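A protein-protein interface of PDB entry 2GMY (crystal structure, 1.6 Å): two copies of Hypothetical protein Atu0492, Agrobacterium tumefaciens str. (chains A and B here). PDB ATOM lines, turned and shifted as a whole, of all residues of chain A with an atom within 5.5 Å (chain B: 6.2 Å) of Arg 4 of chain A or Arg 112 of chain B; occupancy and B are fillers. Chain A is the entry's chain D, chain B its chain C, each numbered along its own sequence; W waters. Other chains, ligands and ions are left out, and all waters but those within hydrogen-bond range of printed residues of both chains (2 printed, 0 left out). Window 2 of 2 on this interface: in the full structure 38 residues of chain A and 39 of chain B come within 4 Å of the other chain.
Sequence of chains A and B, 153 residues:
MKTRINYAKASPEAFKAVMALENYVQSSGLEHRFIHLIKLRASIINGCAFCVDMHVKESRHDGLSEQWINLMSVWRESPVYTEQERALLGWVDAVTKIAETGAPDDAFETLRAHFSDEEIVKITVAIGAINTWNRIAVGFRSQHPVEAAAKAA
Among the printed residues, merely in contact across the chains: Arg 4 of chain A with Trp 91 of chain B (3.9 Å), Arg 4 of chain A with Pro 104 of chain B (3.4 Å), Arg 4 of chain A with Phe 108 of chain B (3.6 Å), Ile 5 of chain A with Phe 108 of chain B (3.9 Å), Ile 5 of chain A with Asp 117 of chain B (3.9 Å), Ile 5 of chain A with Ile 120 of chain B (3.7 Å), Val 138 of chain A with Gly 102 of chain B (3.5 Å), Gly 139 of chain A with Trp 91 of chain B (3.5 Å), Gly 139 of chain A with Ala 103 of chain B (3.9 Å) and Phe 140 of chain A with Ile 120 of chain B (3.5 Å).
The guanidinium group (NH2) of Arg 112 of chain B lies within salt-bridge range of the side-chain carboxylate (OD2) of Asp 117 of chain B.
The guanidinium group (NH1) of Arg 4 of chain A lies within hydrogen-bond range of the backbone carbonyl oxygen (O) of Gly 139 of chain A.
The backbone carbonyl oxygen (O) of Phe 140 of chain A lies within hydrogen-bond range of the backbone NH (N) of Arg 4 of chain A.
O of Val 138 of chain A sits at hydrogen-bond distance from NH1 of Arg 141 of chain A, 2.9 Å away.
Water W1 bridges OD1 of Asp 105 of chain B (3.1 Å) and NE of Arg 4 of chain A (3.2 Å).
Water W2 lies within hydrogen-bond range of the backbone carbonyl oxygen (O) of Gly 102 of chain B (3.3 Å) and the guanidinium group (NH2) of Arg 141 of chain A (3.3 Å).
No position is printed for both chains.
Of the 15 pairs that touch across the chains among the printed residues, none has its exchanged pair printed and touching as well.
Along chain B the printed residues that touch a printed residue of chain A span positions 91 to 120.
Of the 9 printed residues of chain A, 6 touch a printed residue of chain B.
Hydrophobic or aromatic side chains of chain A that line the printed part of chain B: Ile 5, Val 138 and Phe 140.
Among the printed residues, Asp or Glu carboxylates within 4 Å of a Lys or Arg side-chain nitrogen of the other chain: Arg 4 of chain A with Asp 105 of chain B (2.7 Å).
Arg 4 of chain A touches just these residues of chain B: Trp 91 (3.9 Å), Ala 103 (2.8 Å), Pro 104 (3.4 Å), Asp 105 (2.7 Å), Phe 108 (3.6 Å) and Arg 112 (3.2 Å).
Of chain A, only Arg 4 comes within 4 Å of Arg 112 of chain B.
Printed residues of chain B within 4 Å of Phe 140 of chain A: Ile 120.
Printed residues of chain A within 4 Å of Pro 104 of chain B: Arg 4 (3.4 Å).
Of the printed residues of chain A, Asp 117 of chain B touches Ile 5.
Printed residues of chain A within 4 Å of Trp 91 of chain B: Arg 4 (3.9 Å) and Gly 139 (3.5 Å).
Of the printed residues of chain A, Gly 102 of chain B touches Val 138 and Arg 141.
Phe 115 of chain B touches none of the printed residues of chain A.
Ala 107 of chain B touches none of the printed residues of chain A.
The nearest residue of chain B that does not touch Arg 4 of chain A is Asp 117 of chain B (4.8 Å).
The nearest residue of chain A that does not touch Arg 112 of chain B is Ile 5 of chain A (4.1 Å).
The guanidinium group (NH1) of Arg 141 of chain A lies within hydrogen-bond range of the backbone carbonyl oxygen (O) of Gly 102 of chain B.
The backbone carbonyl oxygen (O) of Ala 103 of chain B sits at hydrogen-bond distance from the guanidinium group (NH1) of Arg 4 of chain A, at 2.8 Å.
The guanidinium group (NH2) of Arg 141 of chain A sits at hydrogen-bond distance from the backbone carbonyl oxygen (O) of Ala 103 of chain B (3.1 Å).
NH2 of Arg 4 of chain A is in salt-bridge range of OD1 of Asp 105 of chain B, 2.7 Å away.
NH2 of Arg 112 of chain B is in hydrogen-bond range of O of Arg 4 of chain A, at 3.2 Å.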
ATOM      1  N   LYS A   2       3.077   8.290 -15.679  1.00  0.00           N
ATOM      2  CA  LYS A   2       3.752   7.746 -16.892  1.00  0.00           C
ATOM      3  C   LYS A   2       3.747   8.775 -18.037  1.00  0.00           C
ATOM      4  O   LYS A   2       4.441   8.603 -19.039  1.00  0.00           O
ATOM      5  CB  LYS A   2       3.097   6.430 -17.311  1.00  0.00           C
ATOM      6  CG  LYS A   2       3.091   5.363 -16.205  1.00  0.00           C
ATOM      7  CD  LYS A   2       1.992   4.323 -16.418  1.00  0.00           C
ATOM      8  CE  LYS A   2       2.106   3.188 -15.396  1.00  0.00           C
ATOM      9  NZ  LYS A   2       1.125   2.081 -15.654  1.00  0.00           N
ATOM     10  N   THR A   3       2.984   9.851 -17.854  1.00  0.00           N
ATOM     11  CA  THR A   3       2.866  10.938 -18.830  1.00  0.00           C
ATOM     12  C   THR A   3       4.138  11.795 -18.866  1.00  0.00           C
ATOM     13  O   THR A   3       4.689  12.132 -17.817  1.00  0.00           O
ATOM     14  CB  THR A   3       1.644  11.820 -18.491  1.00  0.00           C
ATOM     15  OG1 THR A   3       0.466  11.001 -18.426  1.00  0.00           O
ATOM     16  CG2 THR A   3       1.451  12.925 -19.518  1.00  0.00           C
ATOM     17  N   ARG A   4       4.600  12.148 -20.065  1.00  0.00           N
ATOM     18  CA  ARG A   4       5.829  12.940 -20.202  1.00  0.00           C
ATOM     19  C   ARG A   4       5.595  14.435 -20.017  1.00  0.00           C
ATOM     20  O   ARG A   4       6.326  15.100 -19.283  1.00  0.00           O
ATOM     21  CB  ARG A   4       6.494  12.695 -21.559  1.00  0.00           C
ATOM     22  CG  ARG A   4       7.178  11.346 -21.667  1.00  0.00           C
ATOM     23  CD  ARG A   4       7.555  11.050 -23.115  1.00  0.00           C
ATOM     24  NE  ARG A   4       8.362   9.829 -23.239  1.00  0.00           N
ATOM     25  CZ  ARG A   4       8.642   9.216 -24.391  1.00  0.00           C
ATOM     26  NH1 ARG A   4       8.174   9.682 -25.548  1.00  0.00           N
ATOM     27  NH2 ARG A   4       9.390   8.125 -24.390  1.00  0.00           N
ATOM     28  N   ILE A   5       4.589  14.951 -20.712  1.00  0.00           N
ATOM     29  CA  ILE A   5       4.233  16.358 -20.660  1.00  0.00           C
ATOM     30  C   ILE A   5       2.717  16.465 -20.666  1.00  0.00           C
ATOM     31  O   ILE A   5       2.040  15.771 -21.429  1.00  0.00           O
ATOM     32  CB  ILE A   5       4.793  17.154 -21.880  1.00  0.00           C
ATOM     33  CG1 ILE A   5       6.323  17.067 -21.944  1.00  0.00           C
ATOM     34  CG2 ILE A   5       4.366  18.626 -21.816  1.00  0.00           C
ATOM     35  CD1 ILE A   5       6.941  17.714 -23.161  1.00  0.00           C
ATOM     36  N   ASN A   6       2.198  17.333 -19.800  1.00  0.00           N
ATOM     37  CA  ASN A   6       0.813  17.772 -19.868  1.00  0.00           C
ATOM     38  C   ASN A   6       0.754  18.844 -20.950  1.00  0.00           C
ATOM     39  O   ASN A   6       0.948  20.039 -20.685  1.00  0.00           O
ATOM     40  CB  ASN A   6       0.381  18.326 -18.510  1.00  0.00           C
ATOM     41  CG  ASN A   6      -1.091  18.707 -18.458  1.00  0.00           C
ATOM     42  OD1 ASN A   6      -1.751  18.884 -19.487  1.00  0.00           O
ATOM     43  ND2 ASN A   6      -1.611  18.844 -17.243  1.00  0.00           N
ATOM     44  N   VAL A 138       1.175   9.435 -28.295  1.00  0.00           N
ATOM     45  CA  VAL A 138       2.270   8.490 -28.091  1.00  0.00           C
ATOM     46  C   VAL A 138       3.535   9.244 -27.680  1.00  0.00           C
ATOM     47  O   VAL A 138       4.231   8.852 -26.737  1.00  0.00           O
ATOM     48  CB  VAL A 138       2.526   7.615 -29.346  1.00  0.00           C
ATOM     49  CG1 VAL A 138       3.728   6.719 -29.125  1.00  0.00           C
ATOM     50  CG2 VAL A 138       1.293   6.758 -29.672  1.00  0.00           C
ATOM     51  N   GLY A 139       3.819  10.344 -28.375  1.00  0.00           N
ATOM     52  CA  GLY A 139       5.014  11.148 -28.103  1.00  0.00           C
ATOM     53  C   GLY A 139       5.090  11.613 -26.662  1.00  0.00           C
ATOM     54  O   GLY A 139       6.172  11.686 -26.081  1.00  0.00           O
ATOM     55  N   PHE A 140       3.940  11.940 -26.080  1.00  0.00           N
ATOM     56  CA  PHE A 140       3.925  12.447 -24.708  1.00  0.00           C
ATOM     57  C   PHE A 140       3.429  11.423 -23.697  1.00  0.00           C
ATOM     58  O   PHE A 140       3.198  11.751 -22.525  1.00  0.00           O
ATOM     59  CB  PHE A 140       3.131  13.749 -24.637  1.00  0.00           C
ATOM     60  CG  PHE A 140       3.726  14.843 -25.481  1.00  0.00           C
ATOM     61  CD1 PHE A 140       5.116  14.956 -25.605  1.00  0.00           C
ATOM     62  CD2 PHE A 140       2.922  15.739 -26.158  1.00  0.00           C
ATOM     63  CE1 PHE A 140       5.694  15.979 -26.389  1.00  0.00           C
ATOM     64  CE2 PHE A 140       3.486  16.757 -26.941  1.00  0.00           C
ATOM     65  CZ  PHE A 140       4.870  16.863 -27.066  1.00  0.00           C
ATOM     66  N   ARG A 141       3.275  10.182 -24.156  1.00  0.00           N
ATOM     67  CA  ARG A 141       2.856   9.068 -23.297  1.00  0.00           C
ATOM     68  C   ARG A 141       1.556   9.353 -22.538  1.00  0.00           C
ATOM     69  O   ARG A 141       1.450   9.072 -21.336  1.00  0.00           O
ATOM     70  CB  ARG A 141       3.995   8.651 -22.348  1.00  0.00           C
ATOM     71  CG  ARG A 141       5.243   8.141 -23.074  1.00  0.00           C
ATOM     72  CD  ARG A 141       5.042   6.731 -23.613  1.00  0.00           C
ATOM     73  NE  ARG A 141       6.295   6.096 -24.041  1.00  0.00           N
ATOM     74  CZ  ARG A 141       6.745   6.067 -25.294  1.00  0.00           C
ATOM     75  NH1 ARG A 141       6.062   6.652 -26.275  1.00  0.00           N
ATOM     76  NH2 ARG A 141       7.892   5.440 -25.572  1.00  0.00           N
ATOM     77  N   TRP B  91      14.088  13.612 -32.913  1.00  0.00           N
ATOM     78  CA  TRP B  91      12.676  13.644 -32.539  1.00  0.00           C
ATOM     79  C   TRP B  91      11.793  13.696 -33.786  1.00  0.00           C
ATOM     80  O   TRP B  91      10.816  12.950 -33.879  1.00  0.00           O
ATOM     81  CB  TRP B  91      12.394  14.830 -31.605  1.00  0.00           C
ATOM     82  CG  TRP B  91      11.016  14.832 -30.968  1.00  0.00           C
ATOM     83  CD1 TRP B  91      10.024  15.750 -31.157  1.00  0.00           C
ATOM     84  CD2 TRP B  91      10.498  13.869 -30.031  1.00  0.00           C
ATOM     85  NE1 TRP B  91       8.912  15.426 -30.401  1.00  0.00           N
ATOM     86  CE2 TRP B  91       9.181  14.281 -29.692  1.00  0.00           C
ATOM     87  CE3 TRP B  91      11.016  12.702 -29.445  1.00  0.00           C
ATOM     88  CZ2 TRP B  91       8.374  13.561 -28.788  1.00  0.00           C
ATOM     89  CZ3 TRP B  91      10.209  11.983 -28.539  1.00  0.00           C
ATOM     90  CH2 TRP B  91       8.903  12.420 -28.222  1.00  0.00           C
ATOM     91  N   GLY B 102       7.658   4.191 -31.903  1.00  0.00           N
ATOM     92  CA  GLY B 102       6.886   4.467 -30.687  1.00  0.00           C
ATOM     93  C   GLY B 102       7.397   5.622 -29.829  1.00  0.00           C
ATOM     94  O   GLY B 102       7.042   5.711 -28.655  1.00  0.00           O
ATOM     95  N   ALA B 103       8.232   6.490 -30.412  1.00  0.00           N
ATOM     96  CA  ALA B 103       8.838   7.675 -29.717  1.00  0.00           C
ATOM     97  C   ALA B 103       9.629   7.368 -28.424  1.00  0.00           C
ATOM     98  O   ALA B 103       9.194   7.705 -27.312  1.00  0.00           O
ATOM     99  CB  ALA B 103       7.810   8.774 -29.487  1.00  0.00           C
ATOM    100  N   PRO B 104      10.809   6.743 -28.580  1.00  0.00           N
ATOM    101  CA  PRO B 104      11.578   6.208 -27.449  1.00  0.00           C
ATOM    102  C   PRO B 104      12.021   7.221 -26.391  1.00  0.00           C
ATOM    103  O   PRO B 104      12.229   8.406 -26.680  1.00  0.00           O
ATOM    104  CB  PRO B 104      12.816   5.586 -28.120  1.00  0.00           C
ATOM    105  CG  PRO B 104      12.440   5.390 -29.549  1.00  0.00           C
ATOM    106  CD  PRO B 104      11.490   6.510 -29.868  1.00  0.00           C
ATOM    107  N   ASP B 105      12.182   6.725 -25.166  1.00  0.00           N
ATOM    108  CA  ASP B 105      12.718   7.516 -24.066  1.00  0.00           C
ATOM    109  C   ASP B 105      13.983   8.287 -24.423  1.00  0.00           C
ATOM    110  O   ASP B 105      14.110   9.465 -24.075  1.00  0.00           O
ATOM    111  CB  ASP B 105      13.015   6.617 -22.859  1.00  0.00           C
ATOM    112  CG  ASP B 105      11.765   6.205 -22.103  1.00  0.00           C
ATOM    113  OD1 ASP B 105      10.657   6.692 -22.428  1.00  0.00           O
ATOM    114  OD2 ASP B 105      11.906   5.392 -21.155  1.00  0.00           O
ATOM    115  N   ASP B 106      14.922   7.630 -25.096  1.00  0.00           N
ATOM    116  CA  ASP B 106      16.212   8.253 -25.383  1.00  0.00           C
ATOM    117  C   ASP B 106      16.074   9.495 -26.272  1.00  0.00           C
ATOM    118  O   ASP B 106      16.674  10.529 -25.981  1.00  0.00           O
ATOM    119  CB  ASP B 106      17.200   7.231 -25.962  1.00  0.00           C
ATOM    120  CG  ASP B 106      17.804   6.319 -24.886  1.00  0.00           C
ATOM    121  OD1 ASP B 106      17.414   6.414 -23.692  1.00  0.00           O
ATOM    122  OD2 ASP B 106      18.682   5.491 -25.238  1.00  0.00           O
ATOM    123  N   ALA B 107      15.255   9.397 -27.323  1.00  0.00           N
ATOM    124  CA  ALA B 107      14.971  10.534 -28.203  1.00  0.00           C
ATOM    125  C   ALA B 107      14.304  11.682 -27.440  1.00  0.00           C
ATOM    126  O   ALA B 107      14.649  12.843 -27.644  1.00  0.00           O
ATOM    127  CB  ALA B 107      14.108  10.101 -29.384  1.00  0.00           C
ATOM    128  N   PHE B 108      13.356  11.353 -26.561  1.00  0.00           N
ATOM    129  CA  PHE B 108      12.640  12.367 -25.792  1.00  0.00           C
ATOM    130  C   PHE B 108      13.561  13.081 -24.801  1.00  0.00           C
ATOM    131  O   PHE B 108      13.540  14.315 -24.696  1.00  0.00           O
ATOM    132  CB  PHE B 108      11.452  11.762 -25.046  1.00  0.00           C
ATOM    133  CG  PHE B 108      10.726  12.754 -24.187  1.00  0.00           C
ATOM    134  CD1 PHE B 108       9.925  13.741 -24.771  1.00  0.00           C
ATOM    135  CD2 PHE B 108      10.865  12.732 -22.797  1.00  0.00           C
ATOM    136  CE1 PHE B 108       9.254  14.678 -23.989  1.00  0.00           C
ATOM    137  CE2 PHE B 108      10.194  13.670 -22.002  1.00  0.00           C
ATOM    138  CZ  PHE B 108       9.399  14.645 -22.590  1.00  0.00           C
ATOM    139  N   GLU B 109      14.372  12.298 -24.091  1.00  0.00           N
ATOM    140  CA  GLU B 109      15.301  12.862 -23.107  1.00  0.00           C
ATOM    141  C   GLU B 109      16.356  13.749 -23.770  1.00  0.00           C
ATOM    142  O   GLU B 109      16.686  14.827 -23.260  1.00  0.00           O
ATOM    143  CB  GLU B 109      15.920  11.757 -22.239  1.00  0.00           C
ATOM    144  CG  GLU B 109      14.901  11.097 -21.305  1.00  0.00           C
ATOM    145  CD  GLU B 109      14.199  12.097 -20.372  1.00  0.00           C
ATOM    146  OE1 GLU B 109      14.878  12.993 -19.812  1.00  0.00           O
ATOM    147  OE2 GLU B 109      12.966  11.988 -20.197  1.00  0.00           O
ATOM    148  N   THR B 110      16.848  13.317 -24.927  1.00  0.00           N
ATOM    149  CA  THR B 110      17.799  14.118 -25.690  1.00  0.00           C
ATOM    150  C   THR B 110      17.165  15.448 -26.100  1.00  0.00           C
ATOM    151  O   THR B 110      17.802  16.497 -26.014  1.00  0.00           O
ATOM    152  CB  THR B 110      18.332  13.353 -26.909  1.00  0.00           C
ATOM    153  OG1 THR B 110      19.004  12.174 -26.454  1.00  0.00           O
ATOM    154  CG2 THR B 110      19.303  14.214 -27.734  1.00  0.00           C
ATOM    155  N   LEU B 111      15.906  15.395 -26.537  1.00  0.00           N
ATOM    156  CA  LEU B 111      15.170  16.607 -26.888  1.00  0.00           C
ATOM    157  C   LEU B 111      14.998  17.549 -25.695  1.00  0.00           C
ATOM    158  O   LEU B 111      15.200  18.764 -25.821  1.00  0.00           O
ATOM    159  CB  LEU B 111      13.798  16.239 -27.454  1.00  0.00           C
ATOM    160  CG  LEU B 111      12.997  17.392 -28.063  1.00  0.00           C
ATOM    161  CD1 LEU B 111      13.636  17.833 -29.375  1.00  0.00           C
ATOM    162  CD2 LEU B 111      11.553  16.960 -28.276  1.00  0.00           C
ATOM    163  N   ARG B 112      14.612  16.975 -24.554  1.00  0.00           N
ATOM    164  CA  ARG B 112      14.445  17.716 -23.300  1.00  0.00           C
ATOM    165  C   ARG B 112      15.700  18.458 -22.837  1.00  0.00           C
ATOM    166  O   ARG B 112      15.597  19.478 -22.154  1.00  0.00           O
ATOM    167  CB  ARG B 112      14.006  16.771 -22.184  1.00  0.00           C
ATOM    168  CG  ARG B 112      12.527  16.613 -22.047  1.00  0.00           C
ATOM    169  CD  ARG B 112      12.210  16.147 -20.639  1.00  0.00           C
ATOM    170  NE  ARG B 112      10.959  16.732 -20.173  1.00  0.00           N
ATOM    171  CZ  ARG B 112      10.168  16.197 -19.246  1.00  0.00           C
ATOM    172  NH1 ARG B 112      10.487  15.040 -18.669  1.00  0.00           N
ATOM    173  NH2 ARG B 112       9.043  16.819 -18.907  1.00  0.00           N
ATOM    174  N   ALA B 113      16.871  17.940 -23.203  1.00  0.00           N
ATOM    175  CA  ALA B 113      18.136  18.560 -22.823  1.00  0.00           C
ATOM    176  C   ALA B 113      18.345  19.897 -23.539  1.00  0.00           C
ATOM    177  O   ALA B 113      19.109  20.744 -23.068  1.00  0.00           O
ATOM    178  CB  ALA B 113      19.290  17.607 -23.116  1.00  0.00           C
ATOM    179  N   HIS B 114      17.639  20.094 -24.657  1.00  0.00           N
ATOM    180  CA  HIS B 114      17.859  21.241 -25.547  1.00  0.00           C
ATOM    181  C   HIS B 114      16.665  22.182 -25.724  1.00  0.00           C
ATOM    182  O   HIS B 114      16.815  23.283 -26.261  1.00  0.00           O
ATOM    183  CB  HIS B 114      18.338  20.749 -26.914  1.00  0.00           C
ATOM    184  CG  HIS B 114      19.671  20.087 -26.863  1.00  0.00           C
ATOM    185  ND1 HIS B 114      20.851  20.801 -26.899  1.00  0.00           N
ATOM    186  CD2 HIS B 114      20.020  18.785 -26.737  1.00  0.00           C
ATOM    187  CE1 HIS B 114      21.868  19.962 -26.817  1.00  0.00           C
ATOM    188  NE2 HIS B 114      21.392  18.734 -26.717  1.00  0.00           N
ATOM    189  N   PHE B 115      15.494  21.743 -25.271  1.00  0.00           N
ATOM    190  CA  PHE B 115      14.248  22.489 -25.435  1.00  0.00           C
ATOM    191  C   PHE B 115      13.379  22.412 -24.191  1.00  0.00           C
ATOM    192  O   PHE B 115      13.365  21.396 -23.496  1.00  0.00           O
ATOM    193  CB  PHE B 115      13.458  21.942 -26.636  1.00  0.00           C
ATOM    194  CG  PHE B 115      14.155  22.125 -27.953  1.00  0.00           C
ATOM    195  CD1 PHE B 115      14.043  23.329 -28.649  1.00  0.00           C
ATOM    196  CD2 PHE B 115      14.905  21.090 -28.511  1.00  0.00           C
ATOM    197  CE1 PHE B 115      14.686  23.506 -29.859  1.00  0.00           C
ATOM    198  CE2 PHE B 115      15.546  21.254 -29.731  1.00  0.00           C
ATOM    199  CZ  PHE B 115      15.436  22.473 -30.407  1.00  0.00           C
ATOM    200  N   SER B 116      12.644  23.490 -23.922  1.00  0.00           N
ATOM    201  CA  SER B 116      11.679  23.516 -22.820  1.00  0.00           C
ATOM    202  C   SER B 116      10.460  22.674 -23.176  1.00  0.00           C
ATOM    203  O   SER B 116      10.208  22.407 -24.361  1.00  0.00           O
ATOM    204  CB  SER B 116      11.209  24.947 -22.552  1.00  0.00           C
ATOM    205  OG  SER B 116      10.414  25.415 -23.631  1.00  0.00           O
ATOM    206  N   ASP B 117       9.685  22.287 -22.165  1.00  0.00           N
ATOM    207  CA  ASP B 117       8.466  21.515 -22.408  1.00  0.00           C
ATOM    208  C   ASP B 117       7.522  22.256 -23.355  1.00  0.00           C
ATOM    209  O   ASP B 117       6.966  21.657 -24.279  1.00  0.00           O
ATOM    210  CB  ASP B 117       7.777  21.143 -21.089  1.00  0.00           C
ATOM    211  CG  ASP B 117       8.488  20.002 -20.363  1.00  0.00           C
ATOM    212  OD1 ASP B 117       9.533  19.526 -20.864  1.00  0.00           O
ATOM    213  OD2 ASP B 117       7.995  19.580 -19.291  1.00  0.00           O
ATOM    214  N   ILE B 120       8.782  21.922 -26.769  1.00  0.00           N
ATOM    215  CA  ILE B 120       8.586  20.533 -27.216  1.00  0.00           C
ATOM    216  C   ILE B 120       7.161  20.308 -27.730  1.00  0.00           C
ATOM    217  O   ILE B 120       6.946  19.616 -28.748  1.00  0.00           O
ATOM    218  CB  ILE B 120       8.977  19.526 -26.119  1.00  0.00           C
ATOM    219  CG1 ILE B 120      10.504  19.569 -25.919  1.00  0.00           C
ATOM    220  CG2 ILE B 120       8.512  18.103 -26.481  1.00  0.00           C
ATOM    221  CD1 ILE B 120      11.002  18.798 -24.706  1.00  0.00           C
HETATM  222  O   HOH W   1      10.466   9.364 -20.819  1.00  0.00           O
HETATM  223  O   HOH W   2       9.393   3.559 -27.882  1.00  0.00           O
